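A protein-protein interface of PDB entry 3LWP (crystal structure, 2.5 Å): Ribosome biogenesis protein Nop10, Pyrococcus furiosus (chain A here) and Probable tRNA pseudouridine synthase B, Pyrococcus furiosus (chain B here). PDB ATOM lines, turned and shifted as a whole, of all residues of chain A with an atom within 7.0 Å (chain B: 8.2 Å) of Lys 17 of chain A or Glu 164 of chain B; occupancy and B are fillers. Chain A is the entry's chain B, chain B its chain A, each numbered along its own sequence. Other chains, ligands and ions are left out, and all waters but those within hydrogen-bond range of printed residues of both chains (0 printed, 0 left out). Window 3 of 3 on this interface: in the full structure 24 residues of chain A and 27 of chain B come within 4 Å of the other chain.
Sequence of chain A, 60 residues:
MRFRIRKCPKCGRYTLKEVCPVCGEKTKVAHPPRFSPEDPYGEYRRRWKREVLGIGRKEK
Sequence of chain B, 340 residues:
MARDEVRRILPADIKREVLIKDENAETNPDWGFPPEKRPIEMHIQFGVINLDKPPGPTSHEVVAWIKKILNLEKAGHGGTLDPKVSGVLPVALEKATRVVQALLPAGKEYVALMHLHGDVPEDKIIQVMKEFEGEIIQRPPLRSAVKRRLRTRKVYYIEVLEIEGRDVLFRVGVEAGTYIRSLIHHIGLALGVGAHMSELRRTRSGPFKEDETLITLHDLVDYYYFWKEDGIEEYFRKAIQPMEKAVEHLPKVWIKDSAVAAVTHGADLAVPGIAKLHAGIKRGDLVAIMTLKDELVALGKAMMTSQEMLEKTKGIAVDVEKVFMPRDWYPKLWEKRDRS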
ATOM      1  N   ARG A   4      25.074 -10.214 -11.460  1.00  0.00           N
ATOM      2  CA  ARG A   4      24.868 -10.781 -10.137  1.00  0.00           C
ATOM      3  C   ARG A   4      26.086 -10.808  -9.177  1.00  0.00           C
ATOM      4  O   ARG A   4      25.911 -10.669  -7.970  1.00  0.00           O
ATOM      5  CB  ARG A   4      24.231 -12.159 -10.275  1.00  0.00           C
ATOM      6  CG  ARG A   4      22.864 -12.102 -10.963  1.00  0.00           C
ATOM      7  CD  ARG A   4      22.044 -13.312 -10.602  1.00  0.00           C
ATOM      8  NE  ARG A   4      21.986 -13.463  -9.146  1.00  0.00           N
ATOM      9  CZ  ARG A   4      21.780 -14.615  -8.518  1.00  0.00           C
ATOM     10  NH1 ARG A   4      21.611 -15.729  -9.215  1.00  0.00           N
ATOM     11  NH2 ARG A   4      21.747 -14.650  -7.196  1.00  0.00           N
ATOM     12  N   ARG A   6      28.887  -9.769  -6.856  1.00  0.00           N
ATOM     13  CA  ARG A   6      29.125  -8.557  -6.085  1.00  0.00           C
ATOM     14  C   ARG A   6      30.437  -8.620  -5.275  1.00  0.00           C
ATOM     15  O   ARG A   6      31.050  -9.687  -5.163  1.00  0.00           O
ATOM     16  CB  ARG A   6      27.936  -8.315  -5.168  1.00  0.00           C
ATOM     17  CG  ARG A   6      26.615  -8.328  -5.896  1.00  0.00           C
ATOM     18  CD  ARG A   6      25.428  -8.103  -4.911  1.00  0.00           C
ATOM     19  NE  ARG A   6      25.497  -6.765  -4.332  1.00  0.00           N
ATOM     20  CZ  ARG A   6      25.055  -5.667  -4.936  1.00  0.00           C
ATOM     21  NH1 ARG A   6      24.491  -5.761  -6.134  1.00  0.00           N
ATOM     22  NH2 ARG A   6      25.176  -4.481  -4.341  1.00  0.00           N
ATOM     23  N   LYS A   7      30.885  -7.492  -4.725  1.00  0.00           N
ATOM     24  CA  LYS A   7      31.979  -7.560  -3.723  1.00  0.00           C
ATOM     25  C   LYS A   7      32.008  -6.546  -2.560  1.00  0.00           C
ATOM     26  O   LYS A   7      31.525  -5.423  -2.699  1.00  0.00           O
ATOM     27  CB  LYS A   7      33.353  -7.704  -4.366  1.00  0.00           C
ATOM     28  CG  LYS A   7      33.662  -6.768  -5.421  1.00  0.00           C
ATOM     29  CD  LYS A   7      35.145  -6.921  -5.779  1.00  0.00           C
ATOM     30  CE  LYS A   7      36.040  -6.919  -4.560  1.00  0.00           C
ATOM     31  NZ  LYS A   7      37.401  -7.503  -4.844  1.00  0.00           N
ATOM     32  N   TYR A  14      33.964 -11.833  -2.603  1.00  0.00           N
ATOM     33  CA  TYR A  14      32.973 -11.941  -3.668  1.00  0.00           C
ATOM     34  C   TYR A  14      31.774 -12.673  -3.096  1.00  0.00           C
ATOM     35  O   TYR A  14      31.930 -13.649  -2.377  1.00  0.00           O
ATOM     36  CB  TYR A  14      33.558 -12.692  -4.868  1.00  0.00           C
ATOM     37  CG  TYR A  14      34.342 -11.789  -5.775  1.00  0.00           C
ATOM     38  CD1 TYR A  14      35.738 -11.726  -5.709  1.00  0.00           C
ATOM     39  CD2 TYR A  14      33.687 -10.959  -6.671  1.00  0.00           C
ATOM     40  CE1 TYR A  14      36.452 -10.874  -6.524  1.00  0.00           C
ATOM     41  CE2 TYR A  14      34.385 -10.102  -7.476  1.00  0.00           C
ATOM     42  CZ  TYR A  14      35.762 -10.059  -7.401  1.00  0.00           C
ATOM     43  OH  TYR A  14      36.419  -9.205  -8.239  1.00  0.00           O
ATOM     44  N   THR A  15      30.584 -12.206  -3.427  1.00  0.00           N
ATOM     45  CA  THR A  15      29.356 -12.743  -2.865  1.00  0.00           C
ATOM     46  C   THR A  15      28.233 -12.389  -3.840  1.00  0.00           C
ATOM     47  O   THR A  15      28.436 -11.507  -4.701  1.00  0.00           O
ATOM     48  CB  THR A  15      29.075 -12.101  -1.484  1.00  0.00           C
ATOM     49  OG1 THR A  15      27.788 -12.462  -1.011  1.00  0.00           O
ATOM     50  CG2 THR A  15      29.093 -10.591  -1.556  1.00  0.00           C
ATOM     51  N   LEU A  16      27.085 -13.082  -3.713  1.00  0.00           N
ATOM     52  CA  LEU A  16      25.812 -12.743  -4.413  1.00  0.00           C
ATOM     53  C   LEU A  16      24.893 -11.897  -3.544  1.00  0.00           C
ATOM     54  O   LEU A  16      23.964 -11.282  -4.044  1.00  0.00           O
ATOM     55  CB  LEU A  16      25.009 -13.999  -4.826  1.00  0.00           C
ATOM     56  CG  LEU A  16      25.729 -14.982  -5.744  1.00  0.00           C
ATOM     57  CD1 LEU A  16      24.770 -16.009  -6.284  1.00  0.00           C
ATOM     58  CD2 LEU A  16      26.369 -14.221  -6.883  1.00  0.00           C
ATOM     59  N   LYS A  17      25.151 -11.908  -2.238  1.00  0.00           N
ATOM     60  CA  LYS A  17      24.416 -11.131  -1.236  1.00  0.00           C
ATOM     61  C   LYS A  17      24.648  -9.596  -1.259  1.00  0.00           C
ATOM     62  O   LYS A  17      25.643  -9.095  -1.819  1.00  0.00           O
ATOM     63  CB  LYS A  17      24.795 -11.662   0.145  1.00  0.00           C
ATOM     64  CG  LYS A  17      24.382 -13.101   0.386  1.00  0.00           C
ATOM     65  CD  LYS A  17      25.297 -13.793   1.405  1.00  0.00           C
ATOM     66  CE  LYS A  17      24.677 -15.083   1.974  1.00  0.00           C
ATOM     67  NZ  LYS A  17      24.062 -15.958   0.921  1.00  0.00           N
ATOM     68  N   GLU A  18      23.751  -8.851  -0.615  1.00  0.00           N
ATOM     69  CA  GLU A  18      23.914  -7.400  -0.509  1.00  0.00           C
ATOM     70  C   GLU A  18      24.722  -6.969   0.721  1.00  0.00           C
ATOM     71  O   GLU A  18      25.304  -5.881   0.728  1.00  0.00           O
ATOM     72  CB  GLU A  18      22.567  -6.680  -0.567  1.00  0.00           C
ATOM     73  CG  GLU A  18      21.913  -6.767  -1.947  1.00  0.00           C
ATOM     74  CD  GLU A  18      20.893  -5.663  -2.211  1.00  0.00           C
ATOM     75  OE1 GLU A  18      21.315  -4.502  -2.442  1.00  0.00           O
ATOM     76  OE2 GLU A  18      19.673  -5.963  -2.214  1.00  0.00           O
ATOM     77  N   VAL A  19      24.762  -7.813   1.754  1.00  0.00           N
ATOM     78  CA  VAL A  19      25.646  -7.554   2.880  1.00  0.00           C
ATOM     79  C   VAL A  19      26.707  -8.656   2.993  1.00  0.00           C
ATOM     80  O   VAL A  19      26.370  -9.835   2.929  1.00  0.00           O
ATOM     81  CB  VAL A  19      24.859  -7.232   4.217  1.00  0.00           C
ATOM     82  CG1 VAL A  19      23.378  -7.272   3.997  1.00  0.00           C
ATOM     83  CG2 VAL A  19      25.276  -8.128   5.411  1.00  0.00           C
ATOM     84  N   CYS A  20      27.980  -8.239   3.081  1.00  0.00           N
ATOM     85  CA  CYS A  20      29.166  -9.108   3.206  1.00  0.00           C
ATOM     86  C   CYS A  20      28.880 -10.116   4.343  1.00  0.00           C
ATOM     87  O   CYS A  20      28.349  -9.742   5.380  1.00  0.00           O
ATOM     88  CB  CYS A  20      30.397  -8.193   3.500  1.00  0.00           C
ATOM     89  SG  CYS A  20      32.286  -8.635   3.399  1.00  0.00           S
ATOM     90  N   PRO A  21      29.177 -11.408   4.128  1.00  0.00           N
ATOM     91  CA  PRO A  21      29.039 -12.434   5.178  1.00  0.00           C
ATOM     92  C   PRO A  21      30.270 -12.560   6.113  1.00  0.00           C
ATOM     93  O   PRO A  21      30.165 -13.104   7.220  1.00  0.00           O
ATOM     94  CB  PRO A  21      28.843 -13.746   4.387  1.00  0.00           C
ATOM     95  CG  PRO A  21      28.767 -13.359   2.942  1.00  0.00           C
ATOM     96  CD  PRO A  21      29.373 -12.003   2.795  1.00  0.00           C
ATOM     97  N   GLU A  25      29.528  -5.284   5.685  1.00  0.00           N
ATOM     98  CA  GLU A  25      29.298  -4.100   4.857  1.00  0.00           C
ATOM     99  C   GLU A  25      28.388  -4.342   3.632  1.00  0.00           C
ATOM    100  O   GLU A  25      28.339  -5.442   3.079  1.00  0.00           O
ATOM    101  CB  GLU A  25      30.631  -3.513   4.381  1.00  0.00           C
ATOM    102  CG  GLU A  25      31.652  -3.301   5.510  1.00  0.00           C
ATOM    103  CD  GLU A  25      31.313  -2.127   6.437  1.00  0.00           C
ATOM    104  OE1 GLU A  25      31.058  -2.359   7.655  1.00  0.00           O
ATOM    105  OE2 GLU A  25      31.306  -0.978   5.937  1.00  0.00           O
ATOM    106  N   LYS A  26      27.668  -3.302   3.215  1.00  0.00           N
ATOM    107  CA  LYS A  26      26.988  -3.321   1.932  1.00  0.00           C
ATOM    108  C   LYS A  26      28.002  -3.637   0.835  1.00  0.00           C
ATOM    109  O   LYS A  26      29.132  -3.160   0.868  1.00  0.00           O
ATOM    110  CB  LYS A  26      26.323  -1.978   1.643  1.00  0.00           C
ATOM    111  CG  LYS A  26      24.899  -1.848   2.176  1.00  0.00           C
ATOM    112  CD  LYS A  26      23.860  -2.207   1.096  1.00  0.00           C
ATOM    113  CE  LYS A  26      22.428  -2.143   1.643  1.00  0.00           C
ATOM    114  NZ  LYS A  26      22.293  -2.888   2.945  1.00  0.00           N
ATOM    115  N   THR A  27      27.593  -4.454  -0.127  1.00  0.00           N
ATOM    116  CA  THR A  27      28.465  -4.855  -1.218  1.00  0.00           C
ATOM    117  C   THR A  27      28.170  -4.020  -2.464  1.00  0.00           C
ATOM    118  O   THR A  27      27.194  -3.283  -2.506  1.00  0.00           O
ATOM    119  CB  THR A  27      28.269  -6.330  -1.558  1.00  0.00           C
ATOM    120  OG1 THR A  27      26.946  -6.511  -2.103  1.00  0.00           O
ATOM    121  CG2 THR A  27      28.450  -7.181  -0.297  1.00  0.00           C
ATOM    122  N   LYS A  28      29.016  -4.156  -3.474  1.00  0.00           N
ATOM    123  CA  LYS A  28      28.835  -3.441  -4.726  1.00  0.00           C
ATOM    124  C   LYS A  28      28.987  -4.371  -5.920  1.00  0.00           C
ATOM    125  O   LYS A  28      29.699  -5.376  -5.861  1.00  0.00           O
ATOM    126  CB  LYS A  28      29.837  -2.283  -4.814  1.00  0.00           C
ATOM    127  CG  LYS A  28      29.190  -0.906  -4.669  1.00  0.00           C
ATOM    128  CD  LYS A  28      29.801  -0.070  -3.556  1.00  0.00           C
ATOM    129  CE  LYS A  28      28.915  -0.110  -2.306  1.00  0.00           C
ATOM    130  NZ  LYS A  28      29.351   0.855  -1.251  1.00  0.00           N
ATOM    131  N   LEU B 113      30.480 -17.414 -12.201  1.00  0.00           N
ATOM    132  CA  LEU B 113      29.125 -17.751 -11.793  1.00  0.00           C
ATOM    133  C   LEU B 113      28.562 -18.857 -12.698  1.00  0.00           C
ATOM    134  O   LEU B 113      28.393 -18.680 -13.911  1.00  0.00           O
ATOM    135  CB  LEU B 113      28.230 -16.527 -11.823  1.00  0.00           C
ATOM    136  CG  LEU B 113      26.839 -16.785 -11.254  1.00  0.00           C
ATOM    137  CD1 LEU B 113      26.951 -17.175  -9.777  1.00  0.00           C
ATOM    138  CD2 LEU B 113      25.993 -15.559 -11.445  1.00  0.00           C
ATOM    139  N   MET B 114      28.293 -20.007 -12.100  1.00  0.00           N
ATOM    140  CA  MET B 114      27.839 -21.160 -12.864  1.00  0.00           C
ATOM    141  C   MET B 114      26.346 -21.415 -12.632  1.00  0.00           C
ATOM    142  O   MET B 114      25.888 -21.437 -11.480  1.00  0.00           O
ATOM    143  CB  MET B 114      28.646 -22.401 -12.499  1.00  0.00           C
ATOM    144  CG  MET B 114      27.937 -23.686 -12.876  1.00  0.00           C
ATOM    145  SD  MET B 114      28.916 -25.176 -12.536  1.00  0.00           S
ATOM    146  CE  MET B 114      28.579 -25.478 -10.800  1.00  0.00           C
ATOM    147  N   HIS B 115      25.591 -21.579 -13.722  1.00  0.00           N
ATOM    148  CA  HIS B 115      24.165 -21.884 -13.606  1.00  0.00           C
ATOM    149  C   HIS B 115      23.848 -23.342 -14.001  1.00  0.00           C
ATOM    150  O   HIS B 115      23.963 -23.736 -15.171  1.00  0.00           O
ATOM    151  CB  HIS B 115      23.340 -20.909 -14.419  1.00  0.00           C
ATOM    152  CG  HIS B 115      21.876 -21.038 -14.179  1.00  0.00           C
ATOM    153  ND1 HIS B 115      21.249 -20.461 -13.096  1.00  0.00           N
ATOM    154  CD2 HIS B 115      20.916 -21.713 -14.856  1.00  0.00           C
ATOM    155  CE1 HIS B 115      19.957 -20.746 -13.134  1.00  0.00           C
ATOM    156  NE2 HIS B 115      19.734 -21.520 -14.180  1.00  0.00           N
ATOM    157  N   LEU B 116      23.493 -24.130 -13.000  1.00  0.00           N
ATOM    158  CA  LEU B 116      23.115 -25.537 -13.171  1.00  0.00           C
ATOM    159  C   LEU B 116      21.760 -25.688 -13.837  1.00  0.00           C
ATOM    160  O   LEU B 116      20.828 -24.961 -13.514  1.00  0.00           O
ATOM    161  CB  LEU B 116      23.043 -26.249 -11.809  1.00  0.00           C
ATOM    162  CG  LEU B 116      24.416 -26.371 -11.137  1.00  0.00           C
ATOM    163  CD1 LEU B 116      24.300 -26.981  -9.743  1.00  0.00           C
ATOM    164  CD2 LEU B 116      25.387 -27.200 -12.026  1.00  0.00           C
ATOM    165  N   GLU B 122      23.855 -29.312  -2.233  1.00  0.00           N
ATOM    166  CA  GLU B 122      25.009 -28.435  -2.053  1.00  0.00           C
ATOM    167  C   GLU B 122      26.282 -29.237  -1.855  1.00  0.00           C
ATOM    168  O   GLU B 122      27.336 -28.873  -2.383  1.00  0.00           O
ATOM    169  CB  GLU B 122      24.790 -27.435  -0.906  1.00  0.00           C
ATOM    170  CG  GLU B 122      23.693 -26.389  -1.198  1.00  0.00           C
ATOM    171  CD  GLU B 122      23.760 -25.159  -0.286  1.00  0.00           C
ATOM    172  OE1 GLU B 122      24.813 -24.939   0.367  1.00  0.00           O
ATOM    173  OE2 GLU B 122      22.757 -24.408  -0.229  1.00  0.00           O
ATOM    174  N   ILE B 125      27.671 -30.842  -5.204  1.00  0.00           N
ATOM    175  CA  ILE B 125      28.339 -29.813  -5.998  1.00  0.00           C
ATOM    176  C   ILE B 125      29.751 -29.598  -5.484  1.00  0.00           C
ATOM    177  O   ILE B 125      30.707 -29.702  -6.241  1.00  0.00           O
ATOM    178  CB  ILE B 125      27.605 -28.473  -5.969  1.00  0.00           C
ATOM    179  CG1 ILE B 125      26.220 -28.609  -6.589  1.00  0.00           C
ATOM    180  CG2 ILE B 125      28.398 -27.409  -6.712  1.00  0.00           C
ATOM    181  CD1 ILE B 125      25.300 -27.452  -6.213  1.00  0.00           C
ATOM    182  N   VAL B 160      34.474 -22.908  -3.617  1.00  0.00           N
ATOM    183  CA  VAL B 160      33.078 -22.571  -3.754  1.00  0.00           C
ATOM    184  C   VAL B 160      32.691 -21.558  -2.693  1.00  0.00           C
ATOM    185  O   VAL B 160      32.608 -21.868  -1.511  1.00  0.00           O
ATOM    186  CB  VAL B 160      32.232 -23.847  -3.706  1.00  0.00           C
ATOM    187  CG1 VAL B 160      30.721 -23.530  -3.476  1.00  0.00           C
ATOM    188  CG2 VAL B 160      32.486 -24.618  -4.992  1.00  0.00           C
ATOM    189  N   LEU B 161      32.491 -20.331  -3.144  1.00  0.00           N
ATOM    190  CA  LEU B 161      32.141 -19.221  -2.281  1.00  0.00           C
ATOM    191  C   LEU B 161      30.691 -19.380  -1.799  1.00  0.00           C
ATOM    192  O   LEU B 161      30.432 -19.416  -0.603  1.00  0.00           O
ATOM    193  CB  LEU B 161      32.332 -17.889  -3.039  1.00  0.00           C
ATOM    194  CG  LEU B 161      33.766 -17.579  -3.517  1.00  0.00           C
ATOM    195  CD1 LEU B 161      33.893 -16.196  -4.126  1.00  0.00           C
ATOM    196  CD2 LEU B 161      34.783 -17.733  -2.369  1.00  0.00           C
ATOM    197  N   GLU B 162      29.756 -19.494  -2.741  1.00  0.00           N
ATOM    198  CA  GLU B 162      28.335 -19.542  -2.421  1.00  0.00           C
ATOM    199  C   GLU B 162      27.513 -20.308  -3.452  1.00  0.00           C
ATOM    200  O   GLU B 162      27.805 -20.312  -4.662  1.00  0.00           O
ATOM    201  CB  GLU B 162      27.759 -18.139  -2.312  1.00  0.00           C
ATOM    202  CG  GLU B 162      28.232 -17.354  -1.108  1.00  0.00           C
ATOM    203  CD  GLU B 162      27.930 -15.860  -1.228  1.00  0.00           C
ATOM    204  OE1 GLU B 162      26.985 -15.497  -1.972  1.00  0.00           O
ATOM    205  OE2 GLU B 162      28.650 -15.058  -0.576  1.00  0.00           O
ATOM    206  N   ILE B 163      26.465 -20.939  -2.944  1.00  0.00           N
ATOM    207  CA  ILE B 163      25.529 -21.674  -3.747  1.00  0.00           C
ATOM    208  C   ILE B 163      24.136 -21.113  -3.457  1.00  0.00           C
ATOM    209  O   ILE B 163      23.774 -20.905  -2.307  1.00  0.00           O
ATOM    210  CB  ILE B 163      25.630 -23.177  -3.434  1.00  0.00           C
ATOM    211  CG1 ILE B 163      27.026 -23.677  -3.831  1.00  0.00           C
ATOM    212  CG2 ILE B 163      24.504 -23.984  -4.157  1.00  0.00           C
ATOM    213  CD1 ILE B 163      27.480 -24.968  -3.115  1.00  0.00           C
ATOM    214  N   GLU B 164      23.380 -20.817  -4.504  1.00  0.00           N
ATOM    215  CA  GLU B 164      22.004 -20.362  -4.339  1.00  0.00           C
ATOM    216  C   GLU B 164      21.068 -21.063  -5.325  1.00  0.00           C
ATOM    217  O   GLU B 164      20.814 -20.564  -6.436  1.00  0.00           O
ATOM    218  CB  GLU B 164      21.902 -18.836  -4.464  1.00  0.00           C
ATOM    219  CG  GLU B 164      22.029 -18.126  -3.117  1.00  0.00           C
ATOM    220  CD  GLU B 164      22.255 -16.620  -3.225  1.00  0.00           C
ATOM    221  OE1 GLU B 164      21.686 -15.968  -4.140  1.00  0.00           O
ATOM    222  OE2 GLU B 164      23.003 -16.085  -2.372  1.00  0.00           O
ATOM    223  N   GLY B 165      20.563 -22.220  -4.895  1.00  0.00           N
ATOM    224  CA  GLY B 165      19.764 -23.086  -5.741  1.00  0.00           C
ATOM    225  C   GLY B 165      20.583 -23.669  -6.872  1.00  0.00           C
ATOM    226  O   GLY B 165      21.388 -24.571  -6.673  1.00  0.00           O
ATOM    227  N   ARG B 166      20.406 -23.133  -8.071  1.00  0.00           N
ATOM    228  CA  ARG B 166      21.218 -23.584  -9.183  1.00  0.00           C
ATOM    229  C   ARG B 166      22.416 -22.668  -9.470  1.00  0.00           C
ATOM    230  O   ARG B 166      23.195 -22.936 -10.400  1.00  0.00           O
ATOM    231  CB  ARG B 166      20.360 -23.751 -10.434  1.00  0.00           C
ATOM    232  CG  ARG B 166      19.219 -24.697 -10.210  1.00  0.00           C
ATOM    233  CD  ARG B 166      18.382 -24.840 -11.442  1.00  0.00           C
ATOM    234  NE  ARG B 166      17.441 -25.921 -11.256  1.00  0.00           N
ATOM    235  CZ  ARG B 166      16.466 -26.212 -12.104  1.00  0.00           C
ATOM    236  NH1 ARG B 166      16.315 -25.494 -13.211  1.00  0.00           N
ATOM    237  NH2 ARG B 166      15.650 -27.226 -11.842  1.00  0.00           N
ATOM    238  N   ASP B 167      22.571 -21.598  -8.689  1.00  0.00           N
ATOM    239  CA  ASP B 167      23.683 -20.673  -8.939  1.00  0.00           C
ATOM    240  C   ASP B 167      24.863 -20.947  -8.022  1.00  0.00           C
ATOM    241  O   ASP B 167      24.761 -20.928  -6.801  1.00  0.00           O
ATOM    242  CB  ASP B 167      23.236 -19.205  -8.920  1.00  0.00           C
ATOM    243  CG  ASP B 167      22.222 -18.891 -10.032  1.00  0.00           C
ATOM    244  OD1 ASP B 167      21.010 -19.171  -9.836  1.00  0.00           O
ATOM    245  OD2 ASP B 167      22.634 -18.369 -11.102  1.00  0.00           O
ATOM    246  N   VAL B 168      25.978 -21.271  -8.631  1.00  0.00           N
ATOM    247  CA  VAL B 168      27.147 -21.592  -7.861  1.00  0.00           C
ATOM    248  C   VAL B 168      28.205 -20.559  -8.150  1.00  0.00           C
ATOM    249  O   VAL B 168      28.643 -20.446  -9.286  1.00  0.00           O
ATOM    250  CB  VAL B 168      27.654 -22.981  -8.234  1.00  0.00           C
ATOM    251  CG1 VAL B 168      28.836 -23.375  -7.328  1.00  0.00           C
ATOM    252  CG2 VAL B 168      26.500 -23.983  -8.153  1.00  0.00           C
ATOM    253  N   LEU B 169      28.602 -19.792  -7.133  1.00  0.00           N
ATOM    254  CA  LEU B 169      29.681 -18.801  -7.294  1.00  0.00           C
ATOM    255  C   LEU B 169      30.985 -19.374  -6.775  1.00  0.00           C
ATOM    256  O   LEU B 169      31.050 -19.866  -5.643  1.00  0.00           O
ATOM    257  CB  LEU B 169      29.362 -17.485  -6.567  1.00  0.00           C
ATOM    258  CG  LEU B 169      30.443 -16.397  -6.598  1.00  0.00           C
ATOM    259  CD1 LEU B 169      30.608 -15.733  -7.979  1.00  0.00           C
ATOM    260  CD2 LEU B 169      30.107 -15.351  -5.558  1.00  0.00           C
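OE2 of Glu 162 of chain B is in hydrogen-bond range of OG1 of Thr 15 of chain A (2.8 Å).
The backbone NH of Leu 16 of chain A is in hydrogen-bond range of the side-chain carboxylate of Glu 162 of chain B (3.0 Å).
OE2 of Glu 164 of chain B lies within salt-bridge range of NZ of Lys 17 of chain A (3.5 Å).
The side-chain carboxylate of Asp 167 of chain B lies within salt-bridge range of the guanidinium group of Arg 4 of chain A, at 3.4 Å.
The side-chain carboxylate (OE1) of Glu 164 of chain B lies within salt-bridge range of the guanidinium group (NH2) of Arg 4 of chain A (3.3 Å).
The backbone NH of Lys 17 of chain A sits at hydrogen-bond distance from the side-chain hydroxyl of Thr 15 of chain A, 3.0 Å away.
The backbone NH of Leu 161 of chain B lies within hydrogen-bond range of the backbone carbonyl oxygen of Leu 169 of chain B.
The backbone carbonyl oxygen (O) of Glu 162 of chain B lies within hydrogen-bond range of the backbone NH (N) of Leu 169 of chain B (2.6 Å).
The backbone NH (N) of Arg 6 of chain A is in hydrogen-bond range of the backbone carbonyl oxygen (O) of Thr 15 of chain A (2.8 Å).
NE of Arg 6 of chain A lies close to O of Lys 17 of chain A (3.4 Å).
ND1 of His 115 of chain B sits at hydrogen-bond distance from OD2 of Asp 167 of chain B.
Among the printed residues, merely in contact across the chains: Tyr 14 of chain A with Leu 161 of chain B, Tyr 14 of chain A with Glu 162 of chain B, Thr 15 of chain A with Leu 169 of chain B, Leu 16 of chain A with Glu 164 of chain B and Pro 21 of chain A with Glu 162 of chain B.
Lys 17 of chain A touches one residue of chain B.
Of chain A, only Arg 4, Leu 16 and Lys 17 come within 4 Å of Glu 164 of chain B.
Printed residues of chain A within 4 Å of Glu 162 of chain B: Tyr 14 (3.998 Å), Thr 15 (2.8 Å), Leu 16 (3.0 Å) and Pro 21 (3.9 Å).
Printed residues of chain A within 4 Å of Leu 161 of chain B: Tyr 14 (3.6 Å).
Of the printed residues of chain B, Tyr 14 of chain A touches Leu 161 (3.6 Å) and Glu 162 (3.998 Å).
Printed residues of chain B within 4 Å of Arg 4 of chain A: Glu 164 and Asp 167.
Of the printed residues of chain A, Leu 169 of chain B touches Thr 15.
Glu 25 of chain A touches none of the printed residues of chain B.
Lys 7 of chain A touches none of the printed residues of chain B.
The nearest printed residue of chain B that does not touch Leu 16 of chain A is Leu 169 of chain B (4.1 Å).
Hydrophobic or aromatic side chains of chain B that line the printed part of chain A: Leu 161 and Leu 169.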
